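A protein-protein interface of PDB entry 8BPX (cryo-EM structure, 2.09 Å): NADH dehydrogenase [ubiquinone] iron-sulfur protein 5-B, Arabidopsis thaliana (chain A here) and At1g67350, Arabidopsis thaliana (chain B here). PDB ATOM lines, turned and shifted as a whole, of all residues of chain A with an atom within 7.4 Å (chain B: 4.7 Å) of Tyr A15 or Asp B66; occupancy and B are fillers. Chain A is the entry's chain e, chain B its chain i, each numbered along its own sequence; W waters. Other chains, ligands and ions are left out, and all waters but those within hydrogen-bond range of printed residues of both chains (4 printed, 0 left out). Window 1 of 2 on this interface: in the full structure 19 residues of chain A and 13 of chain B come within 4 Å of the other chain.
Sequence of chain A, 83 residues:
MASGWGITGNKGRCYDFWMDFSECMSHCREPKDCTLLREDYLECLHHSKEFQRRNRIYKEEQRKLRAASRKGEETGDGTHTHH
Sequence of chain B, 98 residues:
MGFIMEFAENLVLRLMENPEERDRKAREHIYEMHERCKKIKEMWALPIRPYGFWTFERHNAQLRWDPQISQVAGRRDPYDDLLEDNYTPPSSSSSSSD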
ATOM      1  N   ALA A   2     -17.996  15.838  11.851  1.00  0.00           N
ATOM      2  CA  ALA A   2     -17.858  14.373  11.935  1.00  0.00           C
ATOM      3  C   ALA A   2     -16.760  13.709  11.105  1.00  0.00           C
ATOM      4  O   ALA A   2     -16.465  12.641  11.412  1.00  0.00           O
ATOM      5  CB  ALA A   2     -19.225  13.794  11.658  1.00  0.00           C
ATOM      6  N   SER A   3     -16.353  14.332   9.995  1.00  0.00           N
ATOM      7  CA  SER A   3     -15.403  13.688   9.050  1.00  0.00           C
ATOM      8  C   SER A   3     -14.017  13.516   9.667  1.00  0.00           C
ATOM      9  O   SER A   3     -13.328  12.621   9.246  1.00  0.00           O
ATOM     10  CB  SER A   3     -15.324  14.489   7.713  1.00  0.00           C
ATOM     11  OG  SER A   3     -14.450  15.596   7.818  1.00  0.00           O
ATOM     12  N   GLY A   4     -13.604  14.454  10.512  1.00  0.00           N
ATOM     13  CA  GLY A   4     -12.229  14.449  11.033  1.00  0.00           C
ATOM     14  C   GLY A   4     -11.184  15.235  10.257  1.00  0.00           C
ATOM     15  O   GLY A   4     -10.140  15.472  10.804  1.00  0.00           O
ATOM     16  N   TRP A   5     -11.476  15.643   9.007  1.00  0.00           N
ATOM     17  CA  TRP A   5     -10.516  16.424   8.233  1.00  0.00           C
ATOM     18  C   TRP A   5     -10.636  17.894   8.626  1.00  0.00           C
ATOM     19  O   TRP A   5     -11.660  18.533   8.364  1.00  0.00           O
ATOM     20  CB  TRP A   5     -10.752  16.238   6.736  1.00  0.00           C
ATOM     21  CG  TRP A   5     -10.724  14.809   6.245  1.00  0.00           C
ATOM     22  CD1 TRP A   5     -11.800  14.025   5.954  1.00  0.00           C
ATOM     23  CD2 TRP A   5      -9.564  14.014   5.968  1.00  0.00           C
ATOM     24  NE1 TRP A   5     -11.387  12.793   5.518  1.00  0.00           N
ATOM     25  CE2 TRP A   5     -10.019  12.758   5.517  1.00  0.00           C
ATOM     26  CE3 TRP A   5      -8.188  14.242   6.054  1.00  0.00           C
ATOM     27  CZ2 TRP A   5      -9.148  11.734   5.157  1.00  0.00           C
ATOM     28  CZ3 TRP A   5      -7.324  13.224   5.695  1.00  0.00           C
ATOM     29  CH2 TRP A   5      -7.806  11.985   5.252  1.00  0.00           C
ATOM     30  N   LYS A  11      -6.462  17.054  12.748  1.00  0.00           N
ATOM     31  CA  LYS A  11      -7.748  16.529  13.188  1.00  0.00           C
ATOM     32  C   LYS A  11      -8.708  17.673  13.496  1.00  0.00           C
ATOM     33  O   LYS A  11      -8.329  18.671  14.110  1.00  0.00           O
ATOM     34  CB  LYS A  11      -7.572  15.641  14.425  1.00  0.00           C
ATOM     35  CG  LYS A  11      -8.882  15.207  15.070  1.00  0.00           C
ATOM     36  CD  LYS A  11      -8.684  14.705  16.498  1.00  0.00           C
ATOM     37  CE  LYS A  11      -7.739  13.518  16.544  1.00  0.00           C
ATOM     38  NZ  LYS A  11      -8.016  12.552  15.451  1.00  0.00           N
ATOM     39  N   GLY A  12      -9.902  17.536  12.954  1.00  0.00           N
ATOM     40  CA  GLY A  12     -10.965  18.518  13.221  1.00  0.00           C
ATOM     41  C   GLY A  12     -11.183  18.797  14.710  1.00  0.00           C
ATOM     42  O   GLY A  12     -11.044  17.842  15.456  1.00  0.00           O
ATOM     43  N   ARG A  13     -11.660  19.984  15.086  1.00  0.00           N
ATOM     44  CA  ARG A  13     -11.807  20.411  16.476  1.00  0.00           C
ATOM     45  C   ARG A  13     -12.749  19.500  17.255  1.00  0.00           C
ATOM     46  O   ARG A  13     -12.479  19.160  18.411  1.00  0.00           O
ATOM     47  CB  ARG A  13     -12.298  21.861  16.529  1.00  0.00           C
ATOM     48  CG  ARG A  13     -13.004  22.230  17.834  1.00  0.00           C
ATOM     49  CD  ARG A  13     -13.418  23.694  17.885  1.00  0.00           C
ATOM     50  NE  ARG A  13     -14.825  23.890  17.560  1.00  0.00           N
ATOM     51  CZ  ARG A  13     -15.254  24.450  16.437  1.00  0.00           C
ATOM     52  NH1 ARG A  13     -14.408  24.889  15.519  1.00  0.00           N
ATOM     53  NH2 ARG A  13     -16.562  24.578  16.232  1.00  0.00           N
ATOM     54  N   CYS A  14     -13.890  19.141  16.652  1.00  0.00           N
ATOM     55  CA  CYS A  14     -14.994  18.379  17.273  1.00  0.00           C
ATOM     56  C   CYS A  14     -15.014  16.862  16.950  1.00  0.00           C
ATOM     57  O   CYS A  14     -15.908  16.228  17.353  1.00  0.00           O
ATOM     58  CB  CYS A  14     -16.297  19.031  16.840  1.00  0.00           C
ATOM     59  SG  CYS A  14     -16.375  20.784  17.267  1.00  0.00           S
ATOM     60  N   TYR A  15     -14.002  16.347  16.319  1.00  0.00           N
ATOM     61  CA  TYR A  15     -13.911  14.934  15.898  1.00  0.00           C
ATOM     62  C   TYR A  15     -13.777  13.934  17.075  1.00  0.00           C
ATOM     63  O   TYR A  15     -14.438  12.963  16.992  1.00  0.00           O
ATOM     64  CB  TYR A  15     -12.781  14.773  14.889  1.00  0.00           C
ATOM     65  CG  TYR A  15     -12.663  13.362  14.404  1.00  0.00           C
ATOM     66  CD1 TYR A  15     -13.631  12.831  13.572  1.00  0.00           C
ATOM     67  CD2 TYR A  15     -11.629  12.552  14.829  1.00  0.00           C
ATOM     68  CE1 TYR A  15     -13.538  11.534  13.110  1.00  0.00           C
ATOM     69  CE2 TYR A  15     -11.514  11.253  14.376  1.00  0.00           C
ATOM     70  CZ  TYR A  15     -12.471  10.755  13.512  1.00  0.00           C
ATOM     71  OH  TYR A  15     -12.391   9.479  13.090  1.00  0.00           O
ATOM     72  N   ASP A  16     -13.045  14.243  18.131  1.00  0.00           N
ATOM     73  CA  ASP A  16     -12.985  13.320  19.258  1.00  0.00           C
ATOM     74  C   ASP A  16     -14.336  13.214  19.957  1.00  0.00           C
ATOM     75  O   ASP A  16     -14.755  12.116  20.342  1.00  0.00           O
ATOM     76  CB  ASP A  16     -11.882  13.757  20.217  1.00  0.00           C
ATOM     77  CG  ASP A  16     -10.499  13.435  19.682  1.00  0.00           C
ATOM     78  OD1 ASP A  16     -10.401  12.564  18.795  1.00  0.00           O
ATOM     79  OD2 ASP A  16      -9.515  14.056  20.128  1.00  0.00           O
ATOM     80  N   PHE A  17     -15.047  14.336  20.100  1.00  0.00           N
ATOM     81  CA  PHE A  17     -16.402  14.292  20.642  1.00  0.00           C
ATOM     82  C   PHE A  17     -17.315  13.450  19.762  1.00  0.00           C
ATOM     83  O   PHE A  17     -18.104  12.637  20.262  1.00  0.00           O
ATOM     84  CB  PHE A  17     -16.968  15.707  20.770  1.00  0.00           C
ATOM     85  CG  PHE A  17     -16.404  16.493  21.914  1.00  0.00           C
ATOM     86  CD1 PHE A  17     -16.696  16.153  23.223  1.00  0.00           C
ATOM     87  CD2 PHE A  17     -15.597  17.594  21.679  1.00  0.00           C
ATOM     88  CE1 PHE A  17     -16.178  16.886  24.276  1.00  0.00           C
ATOM     89  CE2 PHE A  17     -15.078  18.331  22.727  1.00  0.00           C
ATOM     90  CZ  PHE A  17     -15.367  17.977  24.024  1.00  0.00           C
ATOM     91  N   TRP A  18     -17.221  13.673  18.448  1.00  0.00           N
ATOM     92  CA  TRP A  18     -17.997  12.864  17.501  1.00  0.00           C
ATOM     93  C   TRP A  18     -17.719  11.361  17.710  1.00  0.00           C
ATOM     94  O   TRP A  18     -18.644  10.626  17.664  1.00  0.00           O
ATOM     95  CB  TRP A  18     -17.749  13.280  16.038  1.00  0.00           C
ATOM     96  CG  TRP A  18     -18.405  12.308  15.113  1.00  0.00           C
ATOM     97  CD1 TRP A  18     -17.817  11.338  14.359  1.00  0.00           C
ATOM     98  CD2 TRP A  18     -19.816  12.146  14.945  1.00  0.00           C
ATOM     99  NE1 TRP A  18     -18.768  10.607  13.709  1.00  0.00           N
ATOM    100  CE2 TRP A  18     -20.004  11.081  14.042  1.00  0.00           C
ATOM    101  CE3 TRP A  18     -20.931  12.807  15.460  1.00  0.00           C
ATOM    102  CZ2 TRP A  18     -21.271  10.664  13.651  1.00  0.00           C
ATOM    103  CZ3 TRP A  18     -22.176  12.393  15.069  1.00  0.00           C
ATOM    104  CH2 TRP A  18     -22.347  11.340  14.171  1.00  0.00           C
ATOM    105  N   MET A  19     -16.470  10.999  17.801  1.00  0.00           N
ATOM    106  CA  MET A  19     -16.115   9.588  17.875  1.00  0.00           C
ATOM    107  C   MET A  19     -16.559   8.977  19.198  1.00  0.00           C
ATOM    108  O   MET A  19     -16.998   7.824  19.230  1.00  0.00           O
ATOM    109  CB  MET A  19     -14.613   9.411  17.660  1.00  0.00           C
ATOM    110  CG  MET A  19     -14.170   9.707  16.238  1.00  0.00           C
ATOM    111  SD  MET A  19     -15.133   8.848  14.972  1.00  0.00           S
ATOM    112  CE  MET A  19     -14.471   7.198  15.123  1.00  0.00           C
ATOM    113  N   ASP A  20     -16.469   9.732  20.298  1.00  0.00           N
ATOM    114  CA  ASP A  20     -17.022   9.243  21.560  1.00  0.00           C
ATOM    115  C   ASP A  20     -18.521   9.004  21.443  1.00  0.00           C
ATOM    116  O   ASP A  20     -19.033   7.965  21.876  1.00  0.00           O
ATOM    117  CB  ASP A  20     -16.733  10.221  22.704  1.00  0.00           C
ATOM    118  CG  ASP A  20     -15.283  10.622  22.782  1.00  0.00           C
ATOM    119  OD1 ASP A  20     -14.415   9.755  22.563  1.00  0.00           O
ATOM    120  OD2 ASP A  20     -15.007  11.805  23.080  1.00  0.00           O
ATOM    121  N   PHE A  21     -19.243   9.954  20.841  1.00  0.00           N
ATOM    122  CA  PHE A  21     -20.685   9.789  20.683  1.00  0.00           C
ATOM    123  C   PHE A  21     -21.021   8.585  19.805  1.00  0.00           C
ATOM    124  O   PHE A  21     -21.919   7.799  20.134  1.00  0.00           O
ATOM    125  CB  PHE A  21     -21.287  11.066  20.101  1.00  0.00           C
ATOM    126  CG  PHE A  21     -22.707  10.919  19.653  1.00  0.00           C
ATOM    127  CD1 PHE A  21     -23.704  10.611  20.559  1.00  0.00           C
ATOM    128  CD2 PHE A  21     -23.048  11.100  18.321  1.00  0.00           C
ATOM    129  CE1 PHE A  21     -25.013  10.477  20.147  1.00  0.00           C
ATOM    130  CE2 PHE A  21     -24.358  10.970  17.905  1.00  0.00           C
ATOM    131  CZ  PHE A  21     -25.340  10.660  18.818  1.00  0.00           C
ATOM    132  N   SER A  22     -20.311   8.429  18.685  1.00  0.00           N
ATOM    133  CA  SER A  22     -20.567   7.312  17.781  1.00  0.00           C
ATOM    134  C   SER A  22     -20.260   5.978  18.447  1.00  0.00           C
ATOM    135  O   SER A  22     -21.025   5.017  18.309  1.00  0.00           O
ATOM    136  CB  SER A  22     -19.745   7.467  16.501  1.00  0.00           C
ATOM    137  OG  SER A  22     -20.050   8.679  15.839  1.00  0.00           O
ATOM    138  N   TYR A  41     -20.787  16.929  21.749  1.00  0.00           N
ATOM    139  CA  TYR A  41     -20.497  17.121  20.293  1.00  0.00           C
ATOM    140  C   TYR A  41     -21.176  18.402  19.767  1.00  0.00           C
ATOM    141  O   TYR A  41     -20.474  19.219  19.261  1.00  0.00           O
ATOM    142  CB  TYR A  41     -20.859  15.854  19.508  1.00  0.00           C
ATOM    143  CG  TYR A  41     -20.801  16.072  18.013  1.00  0.00           C
ATOM    144  CD1 TYR A  41     -19.590  16.255  17.376  1.00  0.00           C
ATOM    145  CD2 TYR A  41     -21.955  16.172  17.253  1.00  0.00           C
ATOM    146  CE1 TYR A  41     -19.517  16.477  16.012  1.00  0.00           C
ATOM    147  CE2 TYR A  41     -21.909  16.395  15.887  1.00  0.00           C
ATOM    148  CZ  TYR A  41     -20.679  16.550  15.265  1.00  0.00           C
ATOM    149  OH  TYR A  41     -20.588  16.770  13.930  1.00  0.00           O
ATOM    150  N   CYS A  44     -19.569  21.505  21.100  1.00  0.00           N
ATOM    151  CA  CYS A  44     -18.340  21.792  20.372  1.00  0.00           C
ATOM    152  C   CYS A  44     -18.644  22.434  19.024  1.00  0.00           C
ATOM    153  O   CYS A  44     -17.925  23.337  18.581  1.00  0.00           O
ATOM    154  CB  CYS A  44     -17.515  20.520  20.185  1.00  0.00           C
ATOM    155  SG  CYS A  44     -15.938  20.776  19.337  1.00  0.00           S
ATOM    156  N   LEU A  45     -19.689  22.102  18.334  1.00  0.00           N
ATOM    157  CA  LEU A  45     -19.976  22.695  16.995  1.00  0.00           C
ATOM    158  C   LEU A  45     -20.423  24.142  17.167  1.00  0.00           C
ATOM    159  O   LEU A  45     -19.946  24.957  16.448  1.00  0.00           O
ATOM    160  CB  LEU A  45     -21.123  21.996  16.280  1.00  0.00           C
ATOM    161  CG  LEU A  45     -20.935  20.536  15.862  1.00  0.00           C
ATOM    162  CD1 LEU A  45     -22.132  20.070  15.053  1.00  0.00           C
ATOM    163  CD2 LEU A  45     -19.661  20.312  15.082  1.00  0.00           C
ATOM    164  N   GLN B  62     -17.904   3.811   9.909  1.00  0.00           N
ATOM    165  CA  GLN B  62     -16.874   4.799  10.219  1.00  0.00           C
ATOM    166  C   GLN B  62     -16.049   4.382  11.435  1.00  0.00           C
ATOM    167  O   GLN B  62     -14.840   4.626  11.480  1.00  0.00           O
ATOM    168  CB  GLN B  62     -17.504   6.180  10.425  1.00  0.00           C
ATOM    169  CG  GLN B  62     -16.567   7.214  11.048  1.00  0.00           C
ATOM    170  CD  GLN B  62     -17.157   8.618  11.096  1.00  0.00           C
ATOM    171  OE1 GLN B  62     -18.352   8.799  11.318  1.00  0.00           O
ATOM    172  NE2 GLN B  62     -16.309   9.619  10.895  1.00  0.00           N
ATOM    173  N   ARG B  64     -14.967   1.580  12.125  1.00  0.00           N
ATOM    174  CA  ARG B  64     -13.952   0.614  11.726  1.00  0.00           C
ATOM    175  C   ARG B  64     -13.022   1.125  10.637  1.00  0.00           C
ATOM    176  O   ARG B  64     -11.893   0.637  10.533  1.00  0.00           O
ATOM    177  CB  ARG B  64     -14.612  -0.683  11.249  1.00  0.00           C
ATOM    178  CG  ARG B  64     -15.802  -1.103  12.085  1.00  0.00           C
ATOM    179  CD  ARG B  64     -15.936  -2.613  12.123  1.00  0.00           C
ATOM    180  NE  ARG B  64     -16.271  -3.173  10.820  1.00  0.00           N
ATOM    181  CZ  ARG B  64     -17.443  -3.024  10.216  1.00  0.00           C
ATOM    182  NH1 ARG B  64     -18.423  -2.326  10.765  1.00  0.00           N
ATOM    183  NH2 ARG B  64     -17.636  -3.592   9.029  1.00  0.00           N
ATOM    184  N   TRP B  65     -13.466   2.088   9.828  1.00  0.00           N
ATOM    185  CA  TRP B  65     -12.622   2.624   8.767  1.00  0.00           C
ATOM    186  C   TRP B  65     -11.682   3.699   9.297  1.00  0.00           C
ATOM    187  O   TRP B  65     -10.474   3.645   9.058  1.00  0.00           O
ATOM    188  CB  TRP B  65     -13.491   3.185   7.641  1.00  0.00           C
ATOM    189  CG  TRP B  65     -12.716   3.891   6.574  1.00  0.00           C
ATOM    190  CD1 TRP B  65     -12.764   5.219   6.271  1.00  0.00           C
ATOM    191  CD2 TRP B  65     -11.790   3.303   5.655  1.00  0.00           C
ATOM    192  NE1 TRP B  65     -11.918   5.499   5.228  1.00  0.00           N
ATOM    193  CE2 TRP B  65     -11.307   4.340   4.829  1.00  0.00           C
ATOM    194  CE3 TRP B  65     -11.312   2.006   5.455  1.00  0.00           C
ATOM    195  CZ2 TRP B  65     -10.374   4.117   3.823  1.00  0.00           C
ATOM    196  CZ3 TRP B  65     -10.387   1.786   4.451  1.00  0.00           C
ATOM    197  CH2 TRP B  65      -9.928   2.835   3.648  1.00  0.00           C
ATOM    198  N   ASP B  66     -12.226   4.670  10.027  1.00  0.00           N
ATOM    199  CA  ASP B  66     -11.435   5.809  10.488  1.00  0.00           C
ATOM    200  C   ASP B  66     -10.180   5.430  11.272  1.00  0.00           C
ATOM    201  O   ASP B  66      -9.155   6.109  11.092  1.00  0.00           O
ATOM    202  CB  ASP B  66     -12.329   6.753  11.307  1.00  0.00           C
ATOM    203  CG  ASP B  66     -13.065   7.761  10.434  1.00  0.00           C
ATOM    204  OD1 ASP B  66     -13.041   7.607   9.197  1.00  0.00           O
ATOM    205  OD2 ASP B  66     -13.663   8.708  10.983  1.00  0.00           O
ATOM    206  N   PRO B  67     -10.175   4.413  12.146  1.00  0.00           N
ATOM    207  CA  PRO B  67      -8.898   4.026  12.773  1.00  0.00           C
ATOM    208  C   PRO B  67      -7.829   3.630  11.768  1.00  0.00           C
ATOM    209  O   PRO B  67      -6.640   3.804  12.051  1.00  0.00           O
ATOM    210  CB  PRO B  67      -9.279   2.849  13.683  1.00  0.00           C
ATOM    211  CG  PRO B  67     -10.735   2.966  13.907  1.00  0.00           C
ATOM    212  CD  PRO B  67     -11.329   3.742  12.771  1.00  0.00           C
ATOM    213  N   GLN B  68      -8.217   3.106  10.601  1.00  0.00           N
ATOM    214  CA  GLN B  68      -7.233   2.701   9.603  1.00  0.00           C
ATOM    215  C   GLN B  68      -6.559   3.892   8.926  1.00  0.00           C
ATOM    216  O   GLN B  68      -5.464   3.734   8.378  1.00  0.00           O
ATOM    217  CB  GLN B  68      -7.888   1.802   8.548  1.00  0.00           C
ATOM    218  CG  GLN B  68      -8.310   0.427   9.058  1.00  0.00           C
ATOM    219  CD  GLN B  68      -9.087  -0.369   8.019  1.00  0.00           C
ATOM    220  OE1 GLN B  68      -8.579  -0.663   6.939  1.00  0.00           O
ATOM    221  NE2 GLN B  68     -10.329  -0.711   8.339  1.00  0.00           N
ATOM    222  N   ILE B  69      -7.184   5.069   8.939  1.00  0.00           N
ATOM    223  CA  ILE B  69      -6.607   6.279   8.363  1.00  0.00           C
ATOM    224  C   ILE B  69      -6.206   7.282   9.437  1.00  0.00           C
ATOM    225  O   ILE B  69      -5.974   8.453   9.125  1.00  0.00           O
ATOM    226  CB  ILE B  69      -7.560   6.934   7.348  1.00  0.00           C
ATOM    227  CG1 ILE B  69      -8.949   7.133   7.963  1.00  0.00           C
ATOM    228  CG2 ILE B  69      -7.602   6.132   6.050  1.00  0.00           C
ATOM    229  CD1 ILE B  69      -9.822   8.119   7.216  1.00  0.00           C
ATOM    230  N   SER B  70      -6.115   6.852  10.696  1.00  0.00           N
ATOM    231  CA  SER B  70      -5.882   7.782  11.794  1.00  0.00           C
ATOM    232  C   SER B  70      -4.490   8.403  11.761  1.00  0.00           C
ATOM    233  O   SER B  70      -4.271   9.427  12.412  1.00  0.00           O
ATOM    234  CB  SER B  70      -6.111   7.075  13.134  1.00  0.00           C
ATOM    235  OG  SER B  70      -5.104   6.113  13.379  1.00  0.00           O
ATOM    236  N   ARG B  75      -5.418  14.646   9.120  1.00  0.00           N
ATOM    237  CA  ARG B  75      -6.367  14.375  10.193  1.00  0.00           C
ATOM    238  C   ARG B  75      -5.679  13.922  11.480  1.00  0.00           C
ATOM    239  O   ARG B  75      -6.343  13.371  12.364  1.00  0.00           O
ATOM    240  CB  ARG B  75      -7.401  13.327   9.754  1.00  0.00           C
ATOM    241  CG  ARG B  75      -6.816  11.972   9.403  1.00  0.00           C
ATOM    242  CD  ARG B  75      -7.828  11.106   8.671  1.00  0.00           C
ATOM    243  NE  ARG B  75      -8.904  10.651   9.543  1.00  0.00           N
ATOM    244  CZ  ARG B  75     -10.147  11.108   9.500  1.00  0.00           C
ATOM    245  NH1 ARG B  75     -10.511  12.045   8.639  1.00  0.00           N
ATOM    246  NH2 ARG B  75     -11.049  10.613  10.342  1.00  0.00           N
HETATM  247  O   HOH W   1      -5.992  11.068  13.672  1.00  0.00           O
HETATM  248  O   HOH W   2     -19.880   7.641  13.183  1.00  0.00           O
HETATM  249  O   HOH W   3     -14.000  10.222   7.841  1.00  0.00           O
HETATM  250  O   HOH W   4      -9.561  12.984  12.447  1.00  0.00           O
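Of the printed residues of chain B, Tyr A15 touches Asp B66 and Arg B75.
Of chain A, only Tyr A15 comes within 4 Å of Asp B66.
Printed residues of chain B within 4 Å of Trp A18: Gln B62 (3.0 Å).
Of the printed residues of chain B, Trp A5 touches Arg B75 (3.2 Å).
Printed residues of chain A within 4 Å of Gln B62: Ala A2 (3.1 Å) and Trp A18 (3.0 Å).
Of the printed residues of chain A, Arg B75 touches Ser A3 (2.9 Å), Gly A4 (3.6 Å), Trp A5 (3.2 Å), Lys A11 (3.3 Å) and Tyr A15 (3.3 Å).
The nearest residue of chain B that does not touch Tyr A15 is Gln B62 (4.03 Å).
The nearest residue of chain A that does not touch Asp B66 is Met A19 (4.3 Å).
The nearest printed residue of chain A that does not touch Gln B62 is Tyr A15 (4.03 Å).
NE2 of Gln B62 lies within hydrogen-bond range of O of Ala A2, 3.1 Å away.
The guanidinium group (NH1) of Arg B75 lies within hydrogen-bond range of the backbone carbonyl oxygen (O) of Ser A3 (2.9 Å).
The side-chain carboxylate (OD2) of Asp B66 is in hydrogen-bond range of the side-chain hydroxyl (OH) of Tyr A15, at 2.6 Å.
The side-chain hydroxyl (OH) of Tyr A15 sits at hydrogen-bond distance from the guanidinium group (NH2) of Arg B75 (3.3 Å).
The indole nitrogen of Trp A18 is in hydrogen-bond range of the side-chain amide oxygen of Gln B62 (3.0 Å).
The indole nitrogen (NE1) of Trp A5 sits close to the guanidinium group (NH1) of Arg B75, 3.3 Å away.
Gly A4 touches Arg B75.
Lys A11 touches Arg B75 (CB to O, 3.3 Å).
Of the 19 printed residues of chain A, 7 touch a printed residue of chain B.
Of the 9 printed residues of chain B, 3 touch a printed residue of chain A.
Printed residues of chain B that touch a printed residue of chain A: Gln B62, Asp B66 and Arg B75.
Among the printed residues, 8 pairs touch across the chains.
Among the printed residues, no Asp or Glu carboxylate lies within 4 Å of a Lys or Arg side-chain nitrogen of the other chain.
Water W1 lies within hydrogen-bond range of the backbone carbonyl oxygen of Arg B75 (2.7 Å), the backbone carbonyl oxygen of Ser B70 (2.7 Å) and the side-chain amino group of Lys A11 (3.1 Å).
Water W2 lies within hydrogen-bond range of the side-chain amide oxygen of Gln B62 (2.7 Å), the side-chain hydroxyl of Ser A22 (2.9 Å) and the indole nitrogen of Trp A18 (3.2 Å).
Water W3 bridges the backbone carbonyl oxygen (O) of Ser A3 and the side-chain carboxylate (OD1) of Asp B66.
Water W4 lies within hydrogen-bond range of the backbone carbonyl oxygen (O) of Gly A4 (3.0 Å), the backbone carbonyl oxygen (O) of Arg B75 (3.2 Å) and the side-chain amino group (NZ) of Lys A11 (3.4 Å).
The backbone NH of Trp A5 sits at hydrogen-bond distance from the side-chain hydroxyl of Ser A3, at 3.2 Å.
The backbone carbonyl oxygen (O) of Gly A4 lies within hydrogen-bond range of the backbone NH (N) of Gly A12, at 3.0 Å.
SD of Met A19 lies within hydrogen-bond range of OH of Tyr A15 (3.4 Å).
The side-chain hydroxyl of Ser A22 sits close to the backbone carbonyl oxygen of Trp A18 (3.0 Å).
OD2 of Asp B66 lies within salt-bridge range of NH2 of Arg B75 (3.3 Å).
SG of Cys A14 is disulfide-bonded to SG of Cys A44.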
